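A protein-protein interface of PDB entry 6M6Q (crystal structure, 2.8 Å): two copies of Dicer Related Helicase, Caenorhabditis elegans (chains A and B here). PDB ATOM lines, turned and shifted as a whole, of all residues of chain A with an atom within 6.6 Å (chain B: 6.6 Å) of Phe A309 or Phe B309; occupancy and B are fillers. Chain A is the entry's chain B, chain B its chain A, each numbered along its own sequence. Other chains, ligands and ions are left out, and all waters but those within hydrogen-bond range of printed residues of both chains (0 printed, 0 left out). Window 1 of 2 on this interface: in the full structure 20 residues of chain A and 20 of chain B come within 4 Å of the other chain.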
ATOM      1  N   LYS A 186      14.381  -5.243 -19.771  1.00  0.00           N
ATOM      2  CA  LYS A 186      15.174  -4.973 -18.550  1.00  0.00           C
ATOM      3  C   LYS A 186      15.891  -6.265 -18.120  1.00  0.00           C
ATOM      4  O   LYS A 186      17.088  -6.223 -17.901  1.00  0.00           O
ATOM      5  CB  LYS A 186      14.265  -4.421 -17.452  1.00  0.00           C
ATOM      6  CG  LYS A 186      14.722  -3.097 -16.873  1.00  0.00           C
ATOM      7  CD  LYS A 186      14.082  -2.755 -15.557  1.00  0.00           C
ATOM      8  CE  LYS A 186      12.752  -2.057 -15.704  1.00  0.00           C
ATOM      9  NZ  LYS A 186      12.047  -1.963 -14.403  1.00  0.00           N
ATOM     10  N   ARG A 189      19.113  -7.066 -19.788  1.00  0.00           N
ATOM     11  CA  ARG A 189      20.186  -6.111 -19.387  1.00  0.00           C
ATOM     12  C   ARG A 189      20.735  -6.477 -18.004  1.00  0.00           C
ATOM     13  O   ARG A 189      21.968  -6.480 -17.847  1.00  0.00           O
ATOM     14  CB  ARG A 189      19.680  -4.668 -19.389  1.00  0.00           C
ATOM     15  CG  ARG A 189      19.404  -4.123 -20.783  1.00  0.00           C
ATOM     16  CD  ARG A 189      18.821  -2.720 -20.779  1.00  0.00           C
ATOM     17  NE  ARG A 189      17.911  -2.535 -21.898  1.00  0.00           N
ATOM     18  CZ  ARG A 189      16.599  -2.369 -21.796  1.00  0.00           C
ATOM     19  NH1 ARG A 189      15.869  -2.243 -22.891  1.00  0.00           N
ATOM     20  NH2 ARG A 189      16.015  -2.333 -20.609  1.00  0.00           N
ATOM     21  N   VAL A 190      19.869  -6.724 -17.031  1.00  0.00           N
ATOM     22  CA  VAL A 190      20.292  -6.922 -15.617  1.00  0.00           C
ATOM     23  C   VAL A 190      21.036  -8.263 -15.515  1.00  0.00           C
ATOM     24  O   VAL A 190      22.172  -8.254 -15.034  1.00  0.00           O
ATOM     25  CB  VAL A 190      19.111  -6.832 -14.631  1.00  0.00           C
ATOM     26  CG1 VAL A 190      19.592  -6.851 -13.186  1.00  0.00           C
ATOM     27  CG2 VAL A 190      18.271  -5.593 -14.875  1.00  0.00           C
ATOM     28  N   ALA A 193      24.506  -8.166 -17.226  1.00  0.00           N
ATOM     29  CA  ALA A 193      25.500  -7.287 -16.561  1.00  0.00           C
ATOM     30  C   ALA A 193      25.903  -7.868 -15.197  1.00  0.00           C
ATOM     31  O   ALA A 193      27.026  -7.583 -14.746  1.00  0.00           O
ATOM     32  CB  ALA A 193      24.944  -5.898 -16.414  1.00  0.00           C
ATOM     33  N   ARG A 304      26.652  -3.263  -9.052  1.00  0.00           N
ATOM     34  CA  ARG A 304      26.137  -1.912  -8.718  1.00  0.00           C
ATOM     35  C   ARG A 304      25.679  -1.254 -10.013  1.00  0.00           C
ATOM     36  O   ARG A 304      24.579  -0.707 -10.034  1.00  0.00           O
ATOM     37  CB  ARG A 304      27.232  -1.083  -8.032  1.00  0.00           C
ATOM     38  CG  ARG A 304      26.731  -0.060  -7.021  1.00  0.00           C
ATOM     39  CD  ARG A 304      27.892   0.605  -6.306  1.00  0.00           C
ATOM     40  NE  ARG A 304      28.665   1.488  -7.182  1.00  0.00           N
ATOM     41  CZ  ARG A 304      29.908   1.906  -6.935  1.00  0.00           C
ATOM     42  NH1 ARG A 304      30.545   1.506  -5.847  1.00  0.00           N
ATOM     43  NH2 ARG A 304      30.517   2.709  -7.790  1.00  0.00           N
ATOM     44  N   ALA A 305      26.473  -1.399 -11.070  1.00  0.00           N
ATOM     45  CA  ALA A 305      26.171  -0.877 -12.420  1.00  0.00           C
ATOM     46  C   ALA A 305      24.976  -1.632 -12.996  1.00  0.00           C
ATOM     47  O   ALA A 305      24.108  -0.980 -13.596  1.00  0.00           O
ATOM     48  CB  ALA A 305      27.379  -0.994 -13.315  1.00  0.00           C
ATOM     49  N   ALA A 306      24.905  -2.944 -12.741  1.00  0.00           N
ATOM     50  CA  ALA A 306      23.812  -3.837 -13.180  1.00  0.00           C
ATOM     51  C   ALA A 306      22.493  -3.419 -12.519  1.00  0.00           C
ATOM     52  O   ALA A 306      21.451  -3.573 -13.161  1.00  0.00           O
ATOM     53  CB  ALA A 306      24.159  -5.255 -12.857  1.00  0.00           C
ATOM     54  N   LEU A 307      22.548  -2.908 -11.283  1.00  0.00           N
ATOM     55  CA  LEU A 307      21.358  -2.443 -10.511  1.00  0.00           C
ATOM     56  C   LEU A 307      20.738  -1.219 -11.196  1.00  0.00           C
ATOM     57  O   LEU A 307      19.509  -1.097 -11.135  1.00  0.00           O
ATOM     58  CB  LEU A 307      21.749  -2.100  -9.064  1.00  0.00           C
ATOM     59  CG  LEU A 307      21.805  -3.263  -8.069  1.00  0.00           C
ATOM     60  CD1 LEU A 307      22.268  -2.781  -6.703  1.00  0.00           C
ATOM     61  CD2 LEU A 307      20.460  -3.962  -7.948  1.00  0.00           C
ATOM     62  N   TYR A 308      21.545  -0.332 -11.790  1.00  0.00           N
ATOM     63  CA  TYR A 308      21.056   0.936 -12.414  1.00  0.00           C
ATOM     64  C   TYR A 308      20.235   0.613 -13.672  1.00  0.00           C
ATOM     65  O   TYR A 308      19.384   1.449 -14.046  1.00  0.00           O
ATOM     66  CB  TYR A 308      22.202   1.921 -12.698  1.00  0.00           C
ATOM     67  CG  TYR A 308      22.750   2.601 -11.467  1.00  0.00           C
ATOM     68  CD1 TYR A 308      23.831   2.064 -10.789  1.00  0.00           C
ATOM     69  CD2 TYR A 308      22.139   3.718 -10.919  1.00  0.00           C
ATOM     70  CE1 TYR A 308      24.313   2.631  -9.618  1.00  0.00           C
ATOM     71  CE2 TYR A 308      22.615   4.310  -9.755  1.00  0.00           C
ATOM     72  CZ  TYR A 308      23.709   3.763  -9.100  1.00  0.00           C
ATOM     73  OH  TYR A 308      24.192   4.315  -7.947  1.00  0.00           O
ATOM     74  N   PHE A 309      20.411  -0.583 -14.256  1.00  0.00           N
ATOM     75  CA  PHE A 309      19.546  -1.118 -15.348  1.00  0.00           C
ATOM     76  C   PHE A 309      18.187  -1.534 -14.783  1.00  0.00           C
ATOM     77  O   PHE A 309      17.173  -1.287 -15.442  1.00  0.00           O
ATOM     78  CB  PHE A 309      20.164  -2.345 -16.016  1.00  0.00           C
ATOM     79  CG  PHE A 309      21.376  -2.083 -16.870  1.00  0.00           C
ATOM     80  CD1 PHE A 309      21.257  -1.953 -18.246  1.00  0.00           C
ATOM     81  CD2 PHE A 309      22.645  -2.023 -16.307  1.00  0.00           C
ATOM     82  CE1 PHE A 309      22.375  -1.740 -19.036  1.00  0.00           C
ATOM     83  CE2 PHE A 309      23.760  -1.789 -17.099  1.00  0.00           C
ATOM     84  CZ  PHE A 309      23.624  -1.657 -18.460  1.00  0.00           C
ATOM     85  N   LEU A 310      18.203  -2.224 -13.640  1.00  0.00           N
ATOM     86  CA  LEU A 310      17.008  -2.766 -12.946  1.00  0.00           C
ATOM     87  C   LEU A 310      16.086  -1.619 -12.494  1.00  0.00           C
ATOM     88  O   LEU A 310      14.864  -1.720 -12.733  1.00  0.00           O
ATOM     89  CB  LEU A 310      17.472  -3.601 -11.753  1.00  0.00           C
ATOM     90  CG  LEU A 310      16.363  -4.353 -11.023  1.00  0.00           C
ATOM     91  CD1 LEU A 310      15.847  -5.503 -11.878  1.00  0.00           C
ATOM     92  CD2 LEU A 310      16.840  -4.846  -9.661  1.00  0.00           C
ATOM     93  N   ASP A 311      16.634  -0.589 -11.838  1.00  0.00           N
ATOM     94  CA  ASP A 311      15.856   0.586 -11.358  1.00  0.00           C
ATOM     95  C   ASP A 311      16.791   1.774 -11.176  1.00  0.00           C
ATOM     96  O   ASP A 311      17.659   1.699 -10.284  1.00  0.00           O
ATOM     97  CB  ASP A 311      15.127   0.291 -10.045  1.00  0.00           C
ATOM     98  CG  ASP A 311      14.215   1.420  -9.589  1.00  0.00           C
ATOM     99  OD1 ASP A 311      14.206   1.707  -8.373  1.00  0.00           O
ATOM    100  OD2 ASP A 311      13.479   1.975 -10.455  1.00  0.00           O
ATOM    101  N   LYS A 312      16.502   2.875 -11.879  1.00  0.00           N
ATOM    102  CA  LYS A 312      17.360   4.086 -11.973  1.00  0.00           C
ATOM    103  C   LYS A 312      17.355   4.827 -10.628  1.00  0.00           C
ATOM    104  O   LYS A 312      18.271   5.659 -10.410  1.00  0.00           O
ATOM    105  CB  LYS A 312      16.864   5.003 -13.098  1.00  0.00           C
ATOM    106  CG  LYS A 312      16.511   4.316 -14.416  1.00  0.00           C
ATOM    107  CD  LYS A 312      17.711   4.020 -15.306  1.00  0.00           C
ATOM    108  CE  LYS A 312      17.412   2.999 -16.393  1.00  0.00           C
ATOM    109  NZ  LYS A 312      18.649   2.428 -16.979  1.00  0.00           N
ATOM    110  N   TRP A 314      17.216   3.230  -7.506  1.00  0.00           N
ATOM    111  CA  TRP A 314      17.401   2.157  -6.484  1.00  0.00           C
ATOM    112  C   TRP A 314      18.100   2.704  -5.231  1.00  0.00           C
ATOM    113  O   TRP A 314      17.723   2.313  -4.130  1.00  0.00           O
ATOM    114  CB  TRP A 314      18.083   0.887  -7.048  1.00  0.00           C
ATOM    115  CG  TRP A 314      19.547   1.001  -7.350  1.00  0.00           C
ATOM    116  CD1 TRP A 314      20.106   1.253  -8.568  1.00  0.00           C
ATOM    117  CD2 TRP A 314      20.648   0.819  -6.438  1.00  0.00           C
ATOM    118  NE1 TRP A 314      21.470   1.271  -8.474  1.00  0.00           N
ATOM    119  CE2 TRP A 314      21.832   1.026  -7.177  1.00  0.00           C
ATOM    120  CE3 TRP A 314      20.752   0.550  -5.068  1.00  0.00           C
ATOM    121  CZ2 TRP A 314      23.096   0.961  -6.597  1.00  0.00           C
ATOM    122  CZ3 TRP A 314      22.007   0.489  -4.491  1.00  0.00           C
ATOM    123  CH2 TRP A 314      23.161   0.687  -5.247  1.00  0.00           C
ATOM    124  N   LYS B 186      31.938   1.557 -25.675  1.00  0.00           N
ATOM    125  CA  LYS B 186      31.461   2.407 -24.558  1.00  0.00           C
ATOM    126  C   LYS B 186      30.708   3.607 -25.144  1.00  0.00           C
ATOM    127  O   LYS B 186      29.581   3.841 -24.727  1.00  0.00           O
ATOM    128  CB  LYS B 186      32.629   2.862 -23.680  1.00  0.00           C
ATOM    129  CG  LYS B 186      32.930   1.965 -22.490  1.00  0.00           C
ATOM    130  CD  LYS B 186      33.751   2.640 -21.401  1.00  0.00           C
ATOM    131  CE  LYS B 186      35.238   2.693 -21.699  1.00  0.00           C
ATOM    132  NZ  LYS B 186      35.951   3.621 -20.791  1.00  0.00           N
ATOM    133  N   LEU B 187      31.302   4.283 -26.136  1.00  0.00           N
ATOM    134  CA  LEU B 187      30.743   5.500 -26.790  1.00  0.00           C
ATOM    135  C   LEU B 187      29.292   5.236 -27.238  1.00  0.00           C
ATOM    136  O   LEU B 187      28.420   6.091 -26.974  1.00  0.00           O
ATOM    137  CB  LEU B 187      31.647   5.887 -27.972  1.00  0.00           C
ATOM    138  CG  LEU B 187      31.195   7.093 -28.806  1.00  0.00           C
ATOM    139  CD1 LEU B 187      31.028   8.320 -27.934  1.00  0.00           C
ATOM    140  CD2 LEU B 187      32.180   7.375 -29.934  1.00  0.00           C
ATOM    141  N   ARG B 189      27.125   3.130 -26.148  1.00  0.00           N
ATOM    142  CA  ARG B 189      26.275   2.877 -24.949  1.00  0.00           C
ATOM    143  C   ARG B 189      25.999   4.203 -24.229  1.00  0.00           C
ATOM    144  O   ARG B 189      24.842   4.446 -23.866  1.00  0.00           O
ATOM    145  CB  ARG B 189      26.954   1.895 -23.984  1.00  0.00           C
ATOM    146  CG  ARG B 189      27.647   0.712 -24.651  1.00  0.00           C
ATOM    147  CD  ARG B 189      28.188  -0.323 -23.668  1.00  0.00           C
ATOM    148  NE  ARG B 189      28.102  -1.635 -24.280  1.00  0.00           N
ATOM    149  CZ  ARG B 189      29.111  -2.282 -24.865  1.00  0.00           C
ATOM    150  NH1 ARG B 189      30.340  -1.786 -24.841  1.00  0.00           N
ATOM    151  NH2 ARG B 189      28.881  -3.436 -25.468  1.00  0.00           N
ATOM    152  N   VAL B 190      27.039   5.004 -24.001  1.00  0.00           N
ATOM    153  CA  VAL B 190      26.973   6.254 -23.194  1.00  0.00           C
ATOM    154  C   VAL B 190      26.112   7.270 -23.947  1.00  0.00           C
ATOM    155  O   VAL B 190      25.135   7.739 -23.364  1.00  0.00           O
ATOM    156  CB  VAL B 190      28.375   6.811 -22.902  1.00  0.00           C
ATOM    157  CG1 VAL B 190      28.311   8.082 -22.065  1.00  0.00           C
ATOM    158  CG2 VAL B 190      29.260   5.777 -22.237  1.00  0.00           C
ATOM    159  N   ALA B 193      22.349   6.338 -24.049  1.00  0.00           N
ATOM    160  CA  ALA B 193      21.647   6.381 -22.741  1.00  0.00           C
ATOM    161  C   ALA B 193      21.545   7.826 -22.246  1.00  0.00           C
ATOM    162  O   ALA B 193      20.595   8.123 -21.512  1.00  0.00           O
ATOM    163  CB  ALA B 193      22.352   5.514 -21.722  1.00  0.00           C
ATOM    164  N   ARG B 304      23.033   9.608 -14.752  1.00  0.00           N
ATOM    165  CA  ARG B 304      24.048   8.997 -13.848  1.00  0.00           C
ATOM    166  C   ARG B 304      24.078   7.491 -14.094  1.00  0.00           C
ATOM    167  O   ARG B 304      25.134   6.914 -13.928  1.00  0.00           O
ATOM    168  CB  ARG B 304      23.822   9.346 -12.374  1.00  0.00           C
ATOM    169  CG  ARG B 304      22.600   8.704 -11.752  1.00  0.00           C
ATOM    170  CD  ARG B 304      22.705   8.564 -10.245  1.00  0.00           C
ATOM    171  NE  ARG B 304      21.497   7.947  -9.718  1.00  0.00           N
ATOM    172  CZ  ARG B 304      21.129   7.964  -8.443  1.00  0.00           C
ATOM    173  NH1 ARG B 304      21.888   8.557  -7.532  1.00  0.00           N
ATOM    174  NH2 ARG B 304      19.995   7.388  -8.083  1.00  0.00           N
ATOM    175  N   ALA B 305      22.974   6.909 -14.561  1.00  0.00           N
ATOM    176  CA  ALA B 305      22.902   5.504 -15.024  1.00  0.00           C
ATOM    177  C   ALA B 305      23.714   5.368 -16.319  1.00  0.00           C
ATOM    178  O   ALA B 305      24.343   4.317 -16.521  1.00  0.00           O
ATOM    179  CB  ALA B 305      21.462   5.096 -15.215  1.00  0.00           C
ATOM    180  N   ALA B 306      23.677   6.399 -17.163  1.00  0.00           N
ATOM    181  CA  ALA B 306      24.451   6.505 -18.418  1.00  0.00           C
ATOM    182  C   ALA B 306      25.950   6.585 -18.098  1.00  0.00           C
ATOM    183  O   ALA B 306      26.742   6.072 -18.894  1.00  0.00           O
ATOM    184  CB  ALA B 306      23.988   7.706 -19.208  1.00  0.00           C
ATOM    185  N   LEU B 307      26.316   7.233 -16.987  1.00  0.00           N
ATOM    186  CA  LEU B 307      27.727   7.389 -16.530  1.00  0.00           C
ATOM    187  C   LEU B 307      28.336   6.017 -16.191  1.00  0.00           C
ATOM    188  O   LEU B 307      29.538   5.862 -16.384  1.00  0.00           O
ATOM    189  CB  LEU B 307      27.776   8.307 -15.304  1.00  0.00           C
ATOM    190  CG  LEU B 307      27.997   9.790 -15.580  1.00  0.00           C
ATOM    191  CD1 LEU B 307      27.944  10.578 -14.279  1.00  0.00           C
ATOM    192  CD2 LEU B 307      29.327  10.035 -16.289  1.00  0.00           C
ATOM    193  N   TYR B 308      27.546   5.080 -15.655  1.00  0.00           N
ATOM    194  CA  TYR B 308      28.027   3.745 -15.210  1.00  0.00           C
ATOM    195  C   TYR B 308      28.499   2.916 -16.426  1.00  0.00           C
ATOM    196  O   TYR B 308      29.260   1.961 -16.216  1.00  0.00           O
ATOM    197  CB  TYR B 308      26.959   3.058 -14.350  1.00  0.00           C
ATOM    198  CG  TYR B 308      27.084   3.370 -12.876  1.00  0.00           C
ATOM    199  CD1 TYR B 308      26.429   4.457 -12.306  1.00  0.00           C
ATOM    200  CD2 TYR B 308      27.918   2.618 -12.058  1.00  0.00           C
ATOM    201  CE1 TYR B 308      26.585   4.776 -10.962  1.00  0.00           C
ATOM    202  CE2 TYR B 308      28.080   2.919 -10.712  1.00  0.00           C
ATOM    203  CZ  TYR B 308      27.413   4.002 -10.161  1.00  0.00           C
ATOM    204  OH  TYR B 308      27.569   4.296  -8.834  1.00  0.00           O
ATOM    205  N   PHE B 309      28.098   3.301 -17.646  1.00  0.00           N
ATOM    206  CA  PHE B 309      28.609   2.747 -18.930  1.00  0.00           C
ATOM    207  C   PHE B 309      29.992   3.315 -19.250  1.00  0.00           C
ATOM    208  O   PHE B 309      30.830   2.587 -19.811  1.00  0.00           O
ATOM    209  CB  PHE B 309      27.693   3.106 -20.095  1.00  0.00           C
ATOM    210  CG  PHE B 309      26.369   2.395 -20.129  1.00  0.00           C
ATOM    211  CD1 PHE B 309      26.271   1.100 -20.616  1.00  0.00           C
ATOM    212  CD2 PHE B 309      25.202   3.060 -19.781  1.00  0.00           C
ATOM    213  CE1 PHE B 309      25.038   0.473 -20.706  1.00  0.00           C
ATOM    214  CE2 PHE B 309      23.970   2.428 -19.863  1.00  0.00           C
ATOM    215  CZ  PHE B 309      23.890   1.136 -20.325  1.00  0.00           C
ATOM    216  N   LEU B 310      30.160   4.620 -19.037  1.00  0.00           N
ATOM    217  CA  LEU B 310      31.426   5.369 -19.265  1.00  0.00           C
ATOM    218  C   LEU B 310      32.520   4.842 -18.323  1.00  0.00           C
ATOM    219  O   LEU B 310      33.645   4.643 -18.797  1.00  0.00           O
ATOM    220  CB  LEU B 310      31.148   6.855 -19.030  1.00  0.00           C
ATOM    221  CG  LEU B 310      32.281   7.821 -19.356  1.00  0.00           C
ATOM    222  CD1 LEU B 310      32.620   7.805 -20.842  1.00  0.00           C
ATOM    223  CD2 LEU B 310      31.903   9.228 -18.923  1.00  0.00           C
ATOM    224  N   ASP B 311      32.200   4.632 -17.039  1.00  0.00           N
ATOM    225  CA  ASP B 311      33.139   4.058 -16.034  1.00  0.00           C
ATOM    226  C   ASP B 311      32.349   3.414 -14.896  1.00  0.00           C
ATOM    227  O   ASP B 311      31.388   4.030 -14.428  1.00  0.00           O
ATOM    228  CB  ASP B 311      34.092   5.115 -15.484  1.00  0.00           C
ATOM    229  CG  ASP B 311      35.334   4.525 -14.843  1.00  0.00           C
ATOM    230  OD1 ASP B 311      36.061   3.814 -15.542  1.00  0.00           O
ATOM    231  OD2 ASP B 311      35.547   4.768 -13.643  1.00  0.00           O
ATOM    232  N   LYS B 312      32.729   2.194 -14.510  1.00  0.00           N
ATOM    233  CA  LYS B 312      32.087   1.427 -13.412  1.00  0.00           C
ATOM    234  C   LYS B 312      32.557   1.982 -12.062  1.00  0.00           C
ATOM    235  O   LYS B 312      31.869   1.724 -11.059  1.00  0.00           O
ATOM    236  CB  LYS B 312      32.409  -0.063 -13.538  1.00  0.00           C
ATOM    237  CG  LYS B 312      31.763  -0.758 -14.724  1.00  0.00           C
ATOM    238  CD  LYS B 312      31.906  -2.269 -14.690  1.00  0.00           C
ATOM    239  CE  LYS B 312      31.310  -2.959 -15.904  1.00  0.00           C
ATOM    240  NZ  LYS B 312      32.239  -2.943 -17.061  1.00  0.00           N
ATOM    241  N   TRP B 314      33.333   5.362 -11.469  1.00  0.00           N
ATOM    242  CA  TRP B 314      33.356   6.833 -11.697  1.00  0.00           C
ATOM    243  C   TRP B 314      33.119   7.594 -10.391  1.00  0.00           C
ATOM    244  O   TRP B 314      33.732   8.628 -10.210  1.00  0.00           O
ATOM    245  CB  TRP B 314      32.420   7.299 -12.836  1.00  0.00           C
ATOM    246  CG  TRP B 314      30.957   7.280 -12.533  1.00  0.00           C
ATOM    247  CD1 TRP B 314      30.076   6.320 -12.917  1.00  0.00           C
ATOM    248  CD2 TRP B 314      30.178   8.290 -11.856  1.00  0.00           C
ATOM    249  NE1 TRP B 314      28.815   6.637 -12.502  1.00  0.00           N
ATOM    250  CE2 TRP B 314      28.843   7.830 -11.837  1.00  0.00           C
ATOM    251  CE3 TRP B 314      30.472   9.513 -11.238  1.00  0.00           C
ATOM    252  CZ2 TRP B 314      27.812   8.551 -11.235  1.00  0.00           C
ATOM    253  CZ3 TRP B 314      29.457  10.209 -10.617  1.00  0.00           C
ATOM    254  CH2 TRP B 314      28.145   9.739 -10.628  1.00  0.00           C
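Hydrophobic or aromatic side chains of chain A that line the printed part of chain B: Ala A305, Tyr A308 and Phe A309. Among the printed residues, 8 pairs touch across the chains.
Among the printed residues, merely in contact across the chains: Phe A309 with Phe B309 (3.4 Å), Arg A304 with Lys B312 (3.7 Å), Tyr A308 with Arg B304 (3.8 Å), Ala A305 with Tyr B308 (3.9 Å) and Lys A312 with Ala B305 (3.9 Å).
Of the printed residues of chain B, Arg A304 touches Tyr B308 (3.4 Å) and Lys B312 (3.7 Å). Printed residues of chain B within 4 Å of Ala A305: Tyr B308 (3.9 Å). Phe A309 touches one residue of chain B. Of the printed residues of chain A, Ala B305 touches Lys A312. The nearest residue of chain B that does not touch Phe A309 is Ala B305 (5.9 Å). The nearest residue of chain A that does not touch Phe B309 is Lys A312 (6.1 Å).
O of Lys A312 sits at hydrogen-bond distance from NH2 of Arg B304. OH of Tyr B308 sits at hydrogen-bond distance from OH of Tyr A308 (3.5 Å). OH of Tyr B308 sits at hydrogen-bond distance from NE of Arg A304.
O of Tyr A308 is in hydrogen-bond range of NZ of Lys A312 (3.2 Å).
Arg A304 touches Tyr B308, and with the chains exchanged Tyr A308 touches Arg B304. Arg A304 touches Lys B312, and with the chains exchanged Lys A312 touches Arg B304. Ala A305 touches Tyr B308, but with the chains exchanged Tyr A308 does not touch Ala B305 (4.1 Å). Tyr A308 touches its own counterpart, Tyr B308. Positions printed for both chains: 186, 189, 190, 193, 304, 305, 306, 307, 308, 309, 310, 311, 312 and 314. Of the 8 pairs that touch across the chains among the printed residues, 6 have their exchanged pair printed and touching as well.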
